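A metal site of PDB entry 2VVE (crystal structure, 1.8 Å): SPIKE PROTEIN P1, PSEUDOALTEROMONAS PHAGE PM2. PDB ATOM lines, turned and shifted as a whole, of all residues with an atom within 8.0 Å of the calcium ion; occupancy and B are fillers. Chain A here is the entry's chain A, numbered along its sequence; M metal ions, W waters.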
ATOM      1  N   THR A 149      -5.993  27.692 -16.122  1.00  0.00           N
ATOM      2  CA  THR A 149      -7.354  28.026 -15.721  1.00  0.00           C
ATOM      3  C   THR A 149      -7.305  28.810 -14.408  1.00  0.00           C
ATOM      4  O   THR A 149      -6.631  28.403 -13.459  1.00  0.00           O
ATOM      5  CB  THR A 149      -8.202  26.745 -15.553  1.00  0.00           C
ATOM      6  OG1 THR A 149      -8.178  25.991 -16.772  1.00  0.00           O
ATOM      7  CG2 THR A 149      -9.641  27.073 -15.187  1.00  0.00           C
ATOM      8  N   SER A 150      -7.995  29.953 -14.383  1.00  0.00           N
ATOM      9  CA  SER A 150      -8.066  30.792 -13.191  1.00  0.00           C
ATOM     10  C   SER A 150      -9.215  30.364 -12.290  1.00  0.00           C
ATOM     11  O   SER A 150     -10.389  30.455 -12.685  1.00  0.00           O
ATOM     12  CB  SER A 150      -8.223  32.263 -13.590  1.00  0.00           C
ATOM     13  OG  SER A 150      -7.069  32.744 -14.247  1.00  0.00           O
ATOM     14  N   ILE A 151      -8.867  29.907 -11.097  1.00  0.00           N
ATOM     15  CA  ILE A 151      -9.853  29.493 -10.102  1.00  0.00           C
ATOM     16  C   ILE A 151      -9.939  30.504  -8.965  1.00  0.00           C
ATOM     17  O   ILE A 151      -8.932  30.815  -8.317  1.00  0.00           O
ATOM     18  CB  ILE A 151      -9.545  28.064  -9.550  1.00  0.00           C
ATOM     19  CG1 ILE A 151      -9.666  27.002 -10.654  1.00  0.00           C
ATOM     20  CG2 ILE A 151     -10.439  27.731  -8.344  1.00  0.00           C
ATOM     21  CD1 ILE A 151     -11.038  26.879 -11.329  1.00  0.00           C
ATOM     22  N   SER A 152     -11.143  31.027  -8.729  1.00  0.00           N
ATOM     23  CA  SER A 152     -11.394  31.894  -7.576  1.00  0.00           C
ATOM     24  C   SER A 152     -11.744  31.041  -6.378  1.00  0.00           C
ATOM     25  O   SER A 152     -12.519  30.081  -6.482  1.00  0.00           O
ATOM     26  CB  SER A 152     -12.510  32.906  -7.867  1.00  0.00           C
ATOM     27  OG  SER A 152     -12.127  33.832  -8.863  1.00  0.00           O
ATOM     28  N   VAL A 153     -11.141  31.382  -5.240  1.00  0.00           N
ATOM     29  CA  VAL A 153     -11.363  30.666  -3.990  1.00  0.00           C
ATOM     30  C   VAL A 153     -11.751  31.634  -2.865  1.00  0.00           C
ATOM     31  O   VAL A 153     -11.322  32.790  -2.831  1.00  0.00           O
ATOM     32  CB  VAL A 153     -10.135  29.816  -3.544  1.00  0.00           C
ATOM     33  CG1 VAL A 153      -9.766  28.783  -4.608  1.00  0.00           C
ATOM     34  CG2 VAL A 153      -8.943  30.694  -3.228  1.00  0.00           C
ATOM     35  N   THR A 178      -7.501  34.620  -6.336  1.00  0.00           N
ATOM     36  CA  THR A 178      -7.759  34.177  -7.702  1.00  0.00           C
ATOM     37  C   THR A 178      -6.437  33.942  -8.420  1.00  0.00           C
ATOM     38  O   THR A 178      -5.497  34.747  -8.318  1.00  0.00           O
ATOM     39  CB  THR A 178      -8.643  35.182  -8.473  1.00  0.00           C
ATOM     40  OG1 THR A 178      -9.810  35.490  -7.713  1.00  0.00           O
ATOM     41  CG2 THR A 178      -9.094  34.605  -9.811  1.00  0.00           C
ATOM     42  N   GLY A 179      -6.383  32.837  -9.145  1.00  0.00           N
ATOM     43  CA  GLY A 179      -5.279  32.541 -10.026  1.00  0.00           C
ATOM     44  C   GLY A 179      -5.208  31.063 -10.340  1.00  0.00           C
ATOM     45  O   GLY A 179      -6.171  30.316 -10.077  1.00  0.00           O
ATOM     46  N   GLU A 210     -16.775  29.227  -2.916  1.00  0.00           N
ATOM     47  CA  GLU A 210     -16.788  29.737  -4.281  1.00  0.00           C
ATOM     48  C   GLU A 210     -16.712  28.555  -5.229  1.00  0.00           C
ATOM     49  O   GLU A 210     -15.762  27.779  -5.201  1.00  0.00           O
ATOM     50  CB  GLU A 210     -15.614  30.701  -4.497  1.00  0.00           C
ATOM     51  CG  GLU A 210     -15.533  31.328  -5.882  1.00  0.00           C
ATOM     52  CD  GLU A 210     -16.598  32.377  -6.135  1.00  0.00           C
ATOM     53  OE1 GLU A 210     -16.915  33.154  -5.206  1.00  0.00           O
ATOM     54  OE2 GLU A 210     -17.120  32.422  -7.269  1.00  0.00           O
ATOM     55  N   LEU A 211     -17.760  28.409  -6.055  1.00  0.00           N
ATOM     56  CA  LEU A 211     -17.774  27.400  -7.100  1.00  0.00           C
ATOM     57  C   LEU A 211     -17.511  28.131  -8.425  1.00  0.00           C
ATOM     58  O   LEU A 211     -18.392  28.796  -8.965  1.00  0.00           O
ATOM     59  CB  LEU A 211     -19.118  26.652  -7.108  1.00  0.00           C
ATOM     60  CG  LEU A 211     -19.371  25.571  -8.179  1.00  0.00           C
ATOM     61  CD1 LEU A 211     -18.328  24.470  -8.147  1.00  0.00           C
ATOM     62  CD2 LEU A 211     -20.761  24.990  -8.021  1.00  0.00           C
ATOM     63  N   ASP A 212     -16.274  28.019  -8.901  1.00  0.00           N
ATOM     64  CA  ASP A 212     -15.800  28.796 -10.050  1.00  0.00           C
ATOM     65  C   ASP A 212     -16.434  28.265 -11.342  1.00  0.00           C
ATOM     66  O   ASP A 212     -16.514  27.059 -11.543  1.00  0.00           O
ATOM     67  CB  ASP A 212     -14.269  28.744 -10.124  1.00  0.00           C
ATOM     68  CG  ASP A 212     -13.691  29.703 -11.149  1.00  0.00           C
ATOM     69  OD1 ASP A 212     -13.849  29.441 -12.362  1.00  0.00           O
ATOM     70  OD2 ASP A 212     -13.059  30.708 -10.763  1.00  0.00           O
ATOM     71  N   TYR A 213     -16.888  29.190 -12.187  1.00  0.00           N
ATOM     72  CA  TYR A 213     -17.500  28.857 -13.467  1.00  0.00           C
ATOM     73  C   TYR A 213     -16.653  27.879 -14.289  1.00  0.00           C
ATOM     74  O   TYR A 213     -17.182  26.941 -14.897  1.00  0.00           O
ATOM     75  CB  TYR A 213     -17.772  30.146 -14.258  1.00  0.00           C
ATOM     76  CG  TYR A 213     -18.218  29.955 -15.686  1.00  0.00           C
ATOM     77  CD1 TYR A 213     -19.545  29.666 -15.987  1.00  0.00           C
ATOM     78  CD2 TYR A 213     -17.307  30.067 -16.747  1.00  0.00           C
ATOM     79  CE1 TYR A 213     -19.965  29.486 -17.306  1.00  0.00           C
ATOM     80  CE2 TYR A 213     -17.711  29.893 -18.066  1.00  0.00           C
ATOM     81  CZ  TYR A 213     -19.043  29.603 -18.338  1.00  0.00           C
ATOM     82  OH  TYR A 213     -19.453  29.431 -19.642  1.00  0.00           O
ATOM     83  N   ASP A 214     -15.347  28.119 -14.302  1.00  0.00           N
ATOM     84  CA  ASP A 214     -14.400  27.328 -15.079  1.00  0.00           C
ATOM     85  C   ASP A 214     -14.302  25.881 -14.587  1.00  0.00           C
ATOM     86  O   ASP A 214     -14.101  24.971 -15.395  1.00  0.00           O
ATOM     87  CB  ASP A 214     -13.022  27.986 -15.073  1.00  0.00           C
ATOM     88  CG  ASP A 214     -13.042  29.382 -15.693  1.00  0.00           C
ATOM     89  OD1 ASP A 214     -13.596  29.547 -16.804  1.00  0.00           O
ATOM     90  OD2 ASP A 214     -12.496  30.305 -15.076  1.00  0.00           O
ATOM     91  N   ALA A 215     -14.445  25.698 -13.279  1.00  0.00           N
ATOM     92  CA  ALA A 215     -14.453  24.370 -12.661  1.00  0.00           C
ATOM     93  C   ALA A 215     -15.706  23.596 -13.057  1.00  0.00           C
ATOM     94  O   ALA A 215     -15.643  22.392 -13.302  1.00  0.00           O
ATOM     95  CB  ALA A 215     -14.367  24.486 -11.137  1.00  0.00           C
ATOM     96  N   GLU A 218     -15.180  22.811 -17.130  1.00  0.00           N
ATOM     97  CA  GLU A 218     -14.068  21.917 -17.489  1.00  0.00           C
ATOM     98  C   GLU A 218     -14.143  20.537 -16.840  1.00  0.00           C
ATOM     99  O   GLU A 218     -13.897  19.527 -17.492  1.00  0.00           O
ATOM    100  CB  GLU A 218     -12.717  22.538 -17.117  1.00  0.00           C
ATOM    101  CG  GLU A 218     -12.259  23.679 -18.000  1.00  0.00           C
ATOM    102  CD  GLU A 218     -10.848  24.143 -17.677  1.00  0.00           C
ATOM    103  OE1 GLU A 218      -9.977  23.282 -17.433  1.00  0.00           O
ATOM    104  OE2 GLU A 218     -10.618  25.369 -17.678  1.00  0.00           O
HETATM  105 CA    CA M   1     -12.434  31.436 -13.076  1.00  0.00          CA
HETATM  106  O   HOH W   1     -14.578  32.436 -13.372  1.00  0.00           O
HETATM  107  O   HOH W   2     -11.731  33.107 -14.628  1.00  0.00           O
HETATM  108  O   HOH W   3     -11.579  32.906 -11.877  1.00  0.00           O
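OD2 of Asp 212 lies close to N of Ser 152, at 2.8 Å.
Three residues have an atom within 4 Å of the calcium ion: Ser 150, Asp 212 and Asp 214.
The calcium ion is bound by water W3 (2.1 Å), OD2 of Asp 214 (2.3 Å), O of Ser 150 (2.3 Å), water W1 (2.4 Å), water W2 (2.4 Å), OD2 of Asp 212 (2.5 Å) and OD1 of Asp 212 (2.5 Å).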
